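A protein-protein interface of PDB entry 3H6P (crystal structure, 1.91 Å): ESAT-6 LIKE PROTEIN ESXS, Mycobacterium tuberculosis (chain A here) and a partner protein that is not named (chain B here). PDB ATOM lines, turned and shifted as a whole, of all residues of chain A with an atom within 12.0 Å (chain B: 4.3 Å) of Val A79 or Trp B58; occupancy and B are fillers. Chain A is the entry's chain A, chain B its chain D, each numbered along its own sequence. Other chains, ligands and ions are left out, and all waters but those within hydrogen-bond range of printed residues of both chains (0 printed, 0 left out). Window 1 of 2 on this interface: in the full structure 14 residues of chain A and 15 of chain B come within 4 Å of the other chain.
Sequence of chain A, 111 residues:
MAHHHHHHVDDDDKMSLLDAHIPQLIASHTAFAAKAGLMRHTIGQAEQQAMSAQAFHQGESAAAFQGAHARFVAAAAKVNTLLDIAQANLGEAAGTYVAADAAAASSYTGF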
ATOM      1  N   ALA A  70     -37.041  23.572  22.277  1.00  0.00           N
ATOM      2  CA  ALA A  70     -36.160  23.493  21.124  1.00  0.00           C
ATOM      3  C   ALA A  70     -34.853  22.745  21.459  1.00  0.00           C
ATOM      4  O   ALA A  70     -34.426  21.875  20.691  1.00  0.00           O
ATOM      5  CB  ALA A  70     -35.877  24.922  20.585  1.00  0.00           C
ATOM      6  N   ARG A  71     -34.248  23.046  22.610  1.00  0.00           N
ATOM      7  CA  ARG A  71     -33.007  22.388  23.025  1.00  0.00           C
ATOM      8  C   ARG A  71     -33.213  20.909  23.309  1.00  0.00           C
ATOM      9  O   ARG A  71     -32.338  20.073  23.007  1.00  0.00           O
ATOM     10  CB  ARG A  71     -32.374  23.073  24.238  1.00  0.00           C
ATOM     11  CG  ARG A  71     -31.759  24.428  23.908  1.00  0.00           C
ATOM     12  CD  ARG A  71     -30.903  24.952  25.038  1.00  0.00           C
ATOM     13  NE  ARG A  71     -31.646  25.117  26.288  1.00  0.00           N
ATOM     14  CZ  ARG A  71     -32.383  26.184  26.602  1.00  0.00           C
ATOM     15  NH1 ARG A  71     -32.519  27.193  25.750  1.00  0.00           N
ATOM     16  NH2 ARG A  71     -33.014  26.232  27.774  1.00  0.00           N
ATOM     17  N   PHE A  72     -34.360  20.591  23.893  1.00  0.00           N
ATOM     18  CA  PHE A  72     -34.744  19.203  24.168  1.00  0.00           C
ATOM     19  C   PHE A  72     -34.883  18.377  22.868  1.00  0.00           C
ATOM     20  O   PHE A  72     -34.372  17.256  22.767  1.00  0.00           O
ATOM     21  CB  PHE A  72     -36.067  19.182  24.963  1.00  0.00           C
ATOM     22  CG  PHE A  72     -36.555  17.788  25.300  1.00  0.00           C
ATOM     23  CD1 PHE A  72     -36.258  17.208  26.519  1.00  0.00           C
ATOM     24  CD2 PHE A  72     -37.308  17.065  24.396  1.00  0.00           C
ATOM     25  CE1 PHE A  72     -36.719  15.906  26.829  1.00  0.00           C
ATOM     26  CE2 PHE A  72     -37.753  15.776  24.699  1.00  0.00           C
ATOM     27  CZ  PHE A  72     -37.472  15.216  25.916  1.00  0.00           C
ATOM     28  N   VAL A  73     -35.594  18.934  21.897  1.00  0.00           N
ATOM     29  CA  VAL A  73     -35.785  18.309  20.589  1.00  0.00           C
ATOM     30  C   VAL A  73     -34.429  18.095  19.885  1.00  0.00           C
ATOM     31  O   VAL A  73     -34.167  17.006  19.371  1.00  0.00           O
ATOM     32  CB  VAL A  73     -36.779  19.134  19.751  1.00  0.00           C
ATOM     33  CG1 VAL A  73     -36.796  18.712  18.289  1.00  0.00           C
ATOM     34  CG2 VAL A  73     -38.168  19.016  20.365  1.00  0.00           C
ATOM     35  N   ALA A  74     -33.565  19.102  19.900  1.00  0.00           N
ATOM     36  CA  ALA A  74     -32.227  18.965  19.286  1.00  0.00           C
ATOM     37  C   ALA A  74     -31.429  17.858  19.966  1.00  0.00           C
ATOM     38  O   ALA A  74     -30.816  17.027  19.294  1.00  0.00           O
ATOM     39  CB  ALA A  74     -31.469  20.276  19.343  1.00  0.00           C
ATOM     40  N   ALA A  75     -31.468  17.813  21.301  1.00  0.00           N
ATOM     41  CA  ALA A  75     -30.751  16.773  22.073  1.00  0.00           C
ATOM     42  C   ALA A  75     -31.288  15.369  21.798  1.00  0.00           C
ATOM     43  O   ALA A  75     -30.512  14.414  21.651  1.00  0.00           O
ATOM     44  CB  ALA A  75     -30.815  17.073  23.589  1.00  0.00           C
ATOM     45  N   ALA A  76     -32.609  15.246  21.726  1.00  0.00           N
ATOM     46  CA  ALA A  76     -33.256  13.979  21.410  1.00  0.00           C
ATOM     47  C   ALA A  76     -32.854  13.445  20.027  1.00  0.00           C
ATOM     48  O   ALA A  76     -32.640  12.230  19.860  1.00  0.00           O
ATOM     49  CB  ALA A  76     -34.763  14.112  21.529  1.00  0.00           C
ATOM     50  N   ALA A  77     -32.770  14.330  19.040  1.00  0.00           N
ATOM     51  CA  ALA A  77     -32.271  13.950  17.713  1.00  0.00           C
ATOM     52  C   ALA A  77     -30.859  13.345  17.824  1.00  0.00           C
ATOM     53  O   ALA A  77     -30.554  12.328  17.196  1.00  0.00           O
ATOM     54  CB  ALA A  77     -32.263  15.180  16.773  1.00  0.00           C
ATOM     55  N   LYS A  78     -30.014  13.937  18.661  1.00  0.00           N
ATOM     56  CA  LYS A  78     -28.641  13.442  18.811  1.00  0.00           C
ATOM     57  C   LYS A  78     -28.652  12.086  19.489  1.00  0.00           C
ATOM     58  O   LYS A  78     -27.927  11.193  19.099  1.00  0.00           O
ATOM     59  CB  LYS A  78     -27.790  14.427  19.597  1.00  0.00           C
ATOM     60  CG  LYS A  78     -27.579  15.733  18.876  1.00  0.00           C
ATOM     61  CD  LYS A  78     -26.679  16.671  19.658  1.00  0.00           C
ATOM     62  CE  LYS A  78     -26.905  18.122  19.259  1.00  0.00           C
ATOM     63  NZ  LYS A  78     -26.099  19.055  20.104  1.00  0.00           N
ATOM     64  N   VAL A  79     -29.492  11.946  20.513  1.00  0.00           N
ATOM     65  CA  VAL A  79     -29.640  10.677  21.222  1.00  0.00           C
ATOM     66  C   VAL A  79     -30.086   9.600  20.256  1.00  0.00           C
ATOM     67  O   VAL A  79     -29.552   8.496  20.268  1.00  0.00           O
ATOM     68  CB  VAL A  79     -30.643  10.791  22.421  1.00  0.00           C
ATOM     69  CG1 VAL A  79     -31.075   9.393  22.896  1.00  0.00           C
ATOM     70  CG2 VAL A  79     -30.014  11.603  23.536  1.00  0.00           C
ATOM     71  N   ASN A  80     -31.037   9.914  19.382  1.00  0.00           N
ATOM     72  CA  ASN A  80     -31.478   8.912  18.401  1.00  0.00           C
ATOM     73  C   ASN A  80     -30.384   8.502  17.398  1.00  0.00           C
ATOM     74  O   ASN A  80     -30.208   7.317  17.095  1.00  0.00           O
ATOM     75  CB  ASN A  80     -32.796   9.349  17.733  1.00  0.00           C
ATOM     76  CG  ASN A  80     -33.990   9.054  18.615  1.00  0.00           C
ATOM     77  OD1 ASN A  80     -34.313   7.898  18.844  1.00  0.00           O
ATOM     78  ND2 ASN A  80     -34.626  10.090  19.147  1.00  0.00           N
ATOM     79  N   THR A  81     -29.627   9.470  16.918  1.00  0.00           N
ATOM     80  CA  THR A  81     -28.465   9.199  16.065  1.00  0.00           C
ATOM     81  C   THR A  81     -27.428   8.336  16.772  1.00  0.00           C
ATOM     82  O   THR A  81     -26.901   7.381  16.183  1.00  0.00           O
ATOM     83  CB  THR A  81     -27.806  10.515  15.591  1.00  0.00           C
ATOM     84  OG1 THR A  81     -28.752  11.262  14.804  1.00  0.00           O
ATOM     85  CG2 THR A  81     -26.572  10.216  14.755  1.00  0.00           C
ATOM     86  N   LEU A  82     -27.154   8.654  18.040  1.00  0.00           N
ATOM     87  CA  LEU A  82     -26.160   7.891  18.802  1.00  0.00           C
ATOM     88  C   LEU A  82     -26.635   6.473  19.150  1.00  0.00           C
ATOM     89  O   LEU A  82     -25.808   5.569  19.279  1.00  0.00           O
ATOM     90  CB  LEU A  82     -25.746   8.659  20.059  1.00  0.00           C
ATOM     91  CG  LEU A  82     -24.933   9.903  19.747  1.00  0.00           C
ATOM     92  CD1 LEU A  82     -24.922  10.869  20.928  1.00  0.00           C
ATOM     93  CD2 LEU A  82     -23.500   9.514  19.354  1.00  0.00           C
ATOM     94  N   LEU A  83     -27.944   6.279  19.354  1.00  0.00           N
ATOM     95  CA  LEU A  83     -28.469   4.938  19.594  1.00  0.00           C
ATOM     96  C   LEU A  83     -28.296   4.076  18.343  1.00  0.00           C
ATOM     97  O   LEU A  83     -27.992   2.890  18.425  1.00  0.00           O
ATOM     98  CB  LEU A  83     -29.962   4.979  19.969  1.00  0.00           C
ATOM     99  CG  LEU A  83     -30.338   5.326  21.392  1.00  0.00           C
ATOM    100  CD1 LEU A  83     -31.861   5.457  21.539  1.00  0.00           C
ATOM    101  CD2 LEU A  83     -29.743   4.245  22.314  1.00  0.00           C
ATOM    102  N   ASP A  84     -28.524   4.660  17.176  1.00  0.00           N
ATOM    103  CA  ASP A  84     -28.299   3.922  15.924  1.00  0.00           C
ATOM    104  C   ASP A  84     -26.846   3.523  15.755  1.00  0.00           C
ATOM    105  O   ASP A  84     -26.558   2.386  15.364  1.00  0.00           O
ATOM    106  CB  ASP A  84     -28.767   4.721  14.720  1.00  0.00           C
ATOM    107  CG  ASP A  84     -30.260   4.870  14.678  1.00  0.00           C
ATOM    108  OD1 ASP A  84     -30.957   4.098  15.365  1.00  0.00           O
ATOM    109  OD2 ASP A  84     -30.738   5.791  13.972  1.00  0.00           O
ATOM    110  N   ILE A  85     -25.930   4.437  16.058  1.00  0.00           N
ATOM    111  CA  ILE A  85     -24.508   4.125  16.016  1.00  0.00           C
ATOM    112  C   ILE A  85     -24.150   2.978  16.966  1.00  0.00           C
ATOM    113  O   ILE A  85     -23.412   2.081  16.594  1.00  0.00           O
ATOM    114  CB  ILE A  85     -23.600   5.377  16.309  1.00  0.00           C
ATOM    115  CG1 ILE A  85     -23.725   6.402  15.188  1.00  0.00           C
ATOM    116  CG2 ILE A  85     -22.123   4.948  16.432  1.00  0.00           C
ATOM    117  CD1 ILE A  85     -23.131   7.774  15.511  1.00  0.00           C
ATOM    118  N   ALA A  86     -24.693   3.001  18.177  1.00  0.00           N
ATOM    119  CA  ALA A  86     -24.474   1.941  19.136  1.00  0.00           C
ATOM    120  C   ALA A  86     -24.967   0.623  18.571  1.00  0.00           C
ATOM    121  O   ALA A  86     -24.235  -0.353  18.596  1.00  0.00           O
ATOM    122  CB  ALA A  86     -25.151   2.259  20.465  1.00  0.00           C
ATOM    123  N   GLN A  87     -26.179   0.609  18.018  1.00  0.00           N
ATOM    124  CA  GLN A  87     -26.765  -0.598  17.447  1.00  0.00           C
ATOM    125  C   GLN A  87     -25.903  -1.186  16.323  1.00  0.00           C
ATOM    126  O   GLN A  87     -25.670  -2.408  16.288  1.00  0.00           O
ATOM    127  CB  GLN A  87     -28.197  -0.335  16.936  1.00  0.00           C
ATOM    128  CG  GLN A  87     -28.910  -1.633  16.550  1.00  0.00           C
ATOM    129  CD  GLN A  87     -30.285  -1.455  15.941  1.00  0.00           C
ATOM    130  OE1 GLN A  87     -30.757  -2.342  15.192  1.00  0.00           O
ATOM    131  NE2 GLN A  87     -30.959  -0.381  16.289  1.00  0.00           N
ATOM    132  N   ALA A  88     -25.424  -0.311  15.425  1.00  0.00           N
ATOM    133  CA  ALA A  88     -24.516  -0.704  14.318  1.00  0.00           C
ATOM    134  C   ALA A  88     -23.220  -1.326  14.817  1.00  0.00           C
ATOM    135  O   ALA A  88     -22.594  -2.103  14.103  1.00  0.00           O
ATOM    136  CB  ALA A  88     -24.185   0.515  13.418  1.00  0.00           C
ATOM    137  N   ASN A  89     -22.792  -0.950  16.016  1.00  0.00           N
ATOM    138  CA  ASN A  89     -21.527  -1.428  16.571  1.00  0.00           C
ATOM    139  C   ASN A  89     -21.696  -2.595  17.541  1.00  0.00           C
ATOM    140  O   ASN A  89     -20.752  -2.947  18.269  1.00  0.00           O
ATOM    141  CB  ASN A  89     -20.775  -0.266  17.223  1.00  0.00           C
ATOM    142  CG  ASN A  89     -20.074   0.592  16.205  1.00  0.00           C
ATOM    143  OD1 ASN A  89     -19.056   0.200  15.671  1.00  0.00           O
ATOM    144  ND2 ASN A  89     -20.631   1.743  15.901  1.00  0.00           N
ATOM    145  N   LEU A  90     -22.889  -3.192  17.571  1.00  0.00           N
ATOM    146  CA  LEU A  90     -23.123  -4.387  18.381  1.00  0.00           C
ATOM    147  C   LEU A  90     -22.915  -5.620  17.510  1.00  0.00           C
ATOM    148  O   LEU A  90     -22.278  -6.586  17.939  1.00  0.00           O
ATOM    149  CB  LEU A  90     -24.541  -4.413  18.964  1.00  0.00           C
ATOM    150  CG  LEU A  90     -24.966  -3.367  19.989  1.00  0.00           C
ATOM    151  CD1 LEU A  90     -26.389  -3.675  20.459  1.00  0.00           C
ATOM    152  CD2 LEU A  90     -24.017  -3.286  21.184  1.00  0.00           C
ATOM    153  N   GLY B  29     -29.781   6.303  30.452  1.00  0.00           N
ATOM    154  CA  GLY B  29     -28.623   6.724  29.671  1.00  0.00           C
ATOM    155  C   GLY B  29     -27.337   6.069  30.135  1.00  0.00           C
ATOM    156  O   GLY B  29     -26.538   5.592  29.324  1.00  0.00           O
ATOM    157  N   ILE B  32     -27.305   2.330  29.168  1.00  0.00           N
ATOM    158  CA  ILE B  32     -26.965   2.142  27.758  1.00  0.00           C
ATOM    159  C   ILE B  32     -25.445   2.276  27.512  1.00  0.00           C
ATOM    160  O   ILE B  32     -24.832   1.438  26.833  1.00  0.00           O
ATOM    161  CB  ILE B  32     -27.754   3.107  26.877  1.00  0.00           C
ATOM    162  CG1 ILE B  32     -29.229   2.678  26.888  1.00  0.00           C
ATOM    163  CG2 ILE B  32     -27.177   3.131  25.444  1.00  0.00           C
ATOM    164  CD1 ILE B  32     -30.219   3.687  26.340  1.00  0.00           C
ATOM    165  N   ALA B  33     -24.850   3.312  28.092  1.00  0.00           N
ATOM    166  CA  ALA B  33     -23.413   3.536  27.979  1.00  0.00           C
ATOM    167  C   ALA B  33     -22.597   2.361  28.534  1.00  0.00           C
ATOM    168  O   ALA B  33     -21.605   1.980  27.951  1.00  0.00           O
ATOM    169  CB  ALA B  33     -23.042   4.807  28.693  1.00  0.00           C
ATOM    170  N   TRP B  54     -17.944   8.193  20.795  1.00  0.00           N
ATOM    171  CA  TRP B  54     -19.354   7.914  21.041  1.00  0.00           C
ATOM    172  C   TRP B  54     -19.750   8.196  22.491  1.00  0.00           C
ATOM    173  O   TRP B  54     -20.782   8.822  22.752  1.00  0.00           O
ATOM    174  CB  TRP B  54     -19.676   6.455  20.658  1.00  0.00           C
ATOM    175  CG  TRP B  54     -21.100   6.110  20.910  1.00  0.00           C
ATOM    176  CD1 TRP B  54     -22.120   6.232  20.041  1.00  0.00           C
ATOM    177  CD2 TRP B  54     -21.659   5.609  22.126  1.00  0.00           C
ATOM    178  NE1 TRP B  54     -23.289   5.835  20.629  1.00  0.00           N
ATOM    179  CE2 TRP B  54     -23.038   5.464  21.916  1.00  0.00           C
ATOM    180  CE3 TRP B  54     -21.128   5.283  23.380  1.00  0.00           C
ATOM    181  CZ2 TRP B  54     -23.900   4.978  22.898  1.00  0.00           C
ATOM    182  CZ3 TRP B  54     -21.987   4.810  24.359  1.00  0.00           C
ATOM    183  CH2 TRP B  54     -23.359   4.680  24.113  1.00  0.00           C
ATOM    184  N   GLN B  55     -18.932   7.747  23.437  1.00  0.00           N
ATOM    185  CA  GLN B  55     -19.205   7.921  24.845  1.00  0.00           C
ATOM    186  C   GLN B  55     -19.280   9.391  25.236  1.00  0.00           C
ATOM    187  O   GLN B  55     -20.191   9.813  25.978  1.00  0.00           O
ATOM    188  CB  GLN B  55     -18.124   7.241  25.678  1.00  0.00           C
ATOM    189  CG  GLN B  55     -18.558   6.970  27.087  1.00  0.00           C
ATOM    190  CD  GLN B  55     -17.387   6.800  27.999  1.00  0.00           C
ATOM    191  OE1 GLN B  55     -16.681   7.760  28.289  1.00  0.00           O
ATOM    192  NE2 GLN B  55     -17.147   5.575  28.432  1.00  0.00           N
ATOM    193  N   THR B  56     -18.312  10.162  24.760  1.00  0.00           N
ATOM    194  CA  THR B  56     -18.276  11.613  24.999  1.00  0.00           C
ATOM    195  C   THR B  56     -19.548  12.272  24.459  1.00  0.00           C
ATOM    196  O   THR B  56     -20.194  13.051  25.159  1.00  0.00           O
ATOM    197  CB  THR B  56     -17.033  12.233  24.340  1.00  0.00           C
ATOM    198  OG1 THR B  56     -15.857  11.605  24.876  1.00  0.00           O
ATOM    199  CG2 THR B  56     -16.973  13.739  24.563  1.00  0.00           C
ATOM    200  N   GLN B  57     -19.915  11.938  23.221  1.00  0.00           N
ATOM    201  CA  GLN B  57     -21.104  12.523  22.586  1.00  0.00           C
ATOM    202  C   GLN B  57     -22.396  12.086  23.247  1.00  0.00           C
ATOM    203  O   GLN B  57     -23.355  12.879  23.353  1.00  0.00           O
ATOM    204  CB  GLN B  57     -21.140  12.216  21.087  1.00  0.00           C
ATOM    205  CG  GLN B  57     -20.169  13.061  20.258  1.00  0.00           C
ATOM    206  CD  GLN B  57     -20.197  12.748  18.755  1.00  0.00           C
ATOM    207  OE1 GLN B  57     -19.151  12.582  18.117  1.00  0.00           O
ATOM    208  NE2 GLN B  57     -21.379  12.662  18.197  1.00  0.00           N
ATOM    209  N   TRP B  58     -22.439  10.826  23.686  1.00  0.00           N
ATOM    210  CA  TRP B  58     -23.600  10.290  24.367  1.00  0.00           C
ATOM    211  C   TRP B  58     -23.836  11.010  25.699  1.00  0.00           C
ATOM    212  O   TRP B  58     -24.949  11.456  26.000  1.00  0.00           O
ATOM    213  CB  TRP B  58     -23.415   8.784  24.603  1.00  0.00           C
ATOM    214  CG  TRP B  58     -24.517   8.149  25.334  1.00  0.00           C
ATOM    215  CD1 TRP B  58     -24.525   7.767  26.632  1.00  0.00           C
ATOM    216  CD2 TRP B  58     -25.804   7.820  24.812  1.00  0.00           C
ATOM    217  NE1 TRP B  58     -25.728   7.206  26.957  1.00  0.00           N
ATOM    218  CE2 TRP B  58     -26.542   7.236  25.860  1.00  0.00           C
ATOM    219  CE3 TRP B  58     -26.404   7.961  23.563  1.00  0.00           C
ATOM    220  CZ2 TRP B  58     -27.847   6.775  25.688  1.00  0.00           C
ATOM    221  CZ3 TRP B  58     -27.705   7.523  23.400  1.00  0.00           C
ATOM    222  CH2 TRP B  58     -28.417   6.952  24.456  1.00  0.00           C
ATOM    223  N   ASN B  59     -22.781  11.144  26.487  1.00  0.00           N
ATOM    224  CA  ASN B  59     -22.909  11.783  27.787  1.00  0.00           C
ATOM    225  C   ASN B  59     -23.265  13.263  27.625  1.00  0.00           C
ATOM    226  O   ASN B  59     -24.056  13.784  28.396  1.00  0.00           O
ATOM    227  CB  ASN B  59     -21.640  11.584  28.615  1.00  0.00           C
ATOM    228  CG  ASN B  59     -21.456  10.132  29.063  1.00  0.00           C
ATOM    229  OD1 ASN B  59     -22.415   9.447  29.410  1.00  0.00           O
ATOM    230  ND2 ASN B  59     -20.221   9.679  29.085  1.00  0.00           N
ATOM    231  N   GLN B  60     -22.719  13.921  26.601  1.00  0.00           N
ATOM    232  CA  GLN B  60     -23.060  15.316  26.341  1.00  0.00           C
ATOM    233  C   GLN B  60     -24.516  15.475  25.886  1.00  0.00           C
ATOM    234  O   GLN B  60     -25.198  16.410  26.322  1.00  0.00           O
ATOM    235  CB  GLN B  60     -22.123  15.940  25.307  1.00  0.00           C
ATOM    236  CG  GLN B  60     -22.345  17.445  25.103  1.00  0.00           C
ATOM    237  CD  GLN B  60     -22.215  18.250  26.402  1.00  0.00           C
ATOM    238  OE1 GLN B  60     -21.214  18.142  27.120  1.00  0.00           O
ATOM    239  NE2 GLN B  60     -23.226  19.064  26.702  1.00  0.00           N
ATOM    240  N   ALA B  61     -24.971  14.588  24.996  1.00  0.00           N
ATOM    241  CA  ALA B  61     -26.368  14.576  24.542  1.00  0.00           C
ATOM    242  C   ALA B  61     -27.338  14.372  25.701  1.00  0.00           C
ATOM    243  O   ALA B  61     -28.350  15.053  25.782  1.00  0.00           O
ATOM    244  CB  ALA B  61     -26.597  13.476  23.486  1.00  0.00           C
ATOM    245  N   LEU B  62     -27.032  13.433  26.582  1.00  0.00           N
ATOM    246  CA  LEU B  62     -27.886  13.144  27.745  1.00  0.00           C
ATOM    247  C   LEU B  62     -27.947  14.321  28.702  1.00  0.00           C
ATOM    248  O   LEU B  62     -28.995  14.623  29.249  1.00  0.00           O
ATOM    249  CB  LEU B  62     -27.360  11.957  28.526  1.00  0.00           C
ATOM    250  CG  LEU B  62     -27.798  10.577  28.094  1.00  0.00           C
ATOM    251  CD1 LEU B  62     -27.740  10.425  26.600  1.00  0.00           C
ATOM    252  CD2 LEU B  62     -26.890   9.582  28.792  1.00  0.00           C
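The backbone carbonyl oxygen (O) of Leu A82 lies within hydrogen-bond range of the indole nitrogen (NE1) of Trp B54, at 2.9 Å.
Hydrophobic or aromatic side chains of chain B that line the printed part of chain A: Trp B54, Trp B58, Ala B61 and Leu B62.
Among the printed residues, merely in contact across the chains: Leu A82 with Gln B57 (3.5 Å), Leu A82 with Trp B58 (3.6 Å), Leu A83 with Trp B58 (3.7 Å), Val A79 with Trp B58 (3.8 Å), Ile A85 with Trp B54 (3.8 Å), Ala A86 with Trp B54 (3.9 Å), Ala A75 with Ala B61 (3.9 Å), Val A79 with Ala B61 (3.9 Å) and Val A79 with Leu B62 (3.99 Å).
The backbone carbonyl oxygen (O) of Gly B29 sits at hydrogen-bond distance from the indole nitrogen (NE1) of Trp B58, 3.0 Å away.
The backbone carbonyl oxygen of Ile A85 sits at hydrogen-bond distance from the side-chain amide nitrogen of Asn A89 (2.9 Å).
Of the printed residues of chain B, Val A79 touches Trp B58 (3.8 Å), Ala B61 (3.9 Å) and Leu B62 (3.99 Å).
Gly B29 touches none of the printed residues of chain A.
No residue of chain A comes within 4 Å of Ala B33.
Trp B54 touches just these residues of chain A: Leu A82 (2.9 Å), Ile A85 (3.8 Å) and Ala A86 (3.9 Å).
Gln B55 touches none of the printed residues of chain A.
No residue of chain A comes within 4 Å of Thr B56.
Printed residues of chain A within 4 Å of Gln B57: Leu A82 (3.5 Å).
No residue of chain A comes within 4 Å of Gln B60.
Of the printed residues of chain B, Ile A85 touches Trp B54.
Of the printed residues of chain B, Leu A82 touches Trp B54, Gln B57 and Trp B58.
Of the printed residues of chain B, Ala A86 touches Trp B54 (3.9 Å).
Of the printed residues of chain A, Ala B61 touches Ala A75 (3.9 Å) and Val A79 (3.9 Å).
The nearest residue of chain A that does not touch Trp B58 is Lys A78 (5.7 Å).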
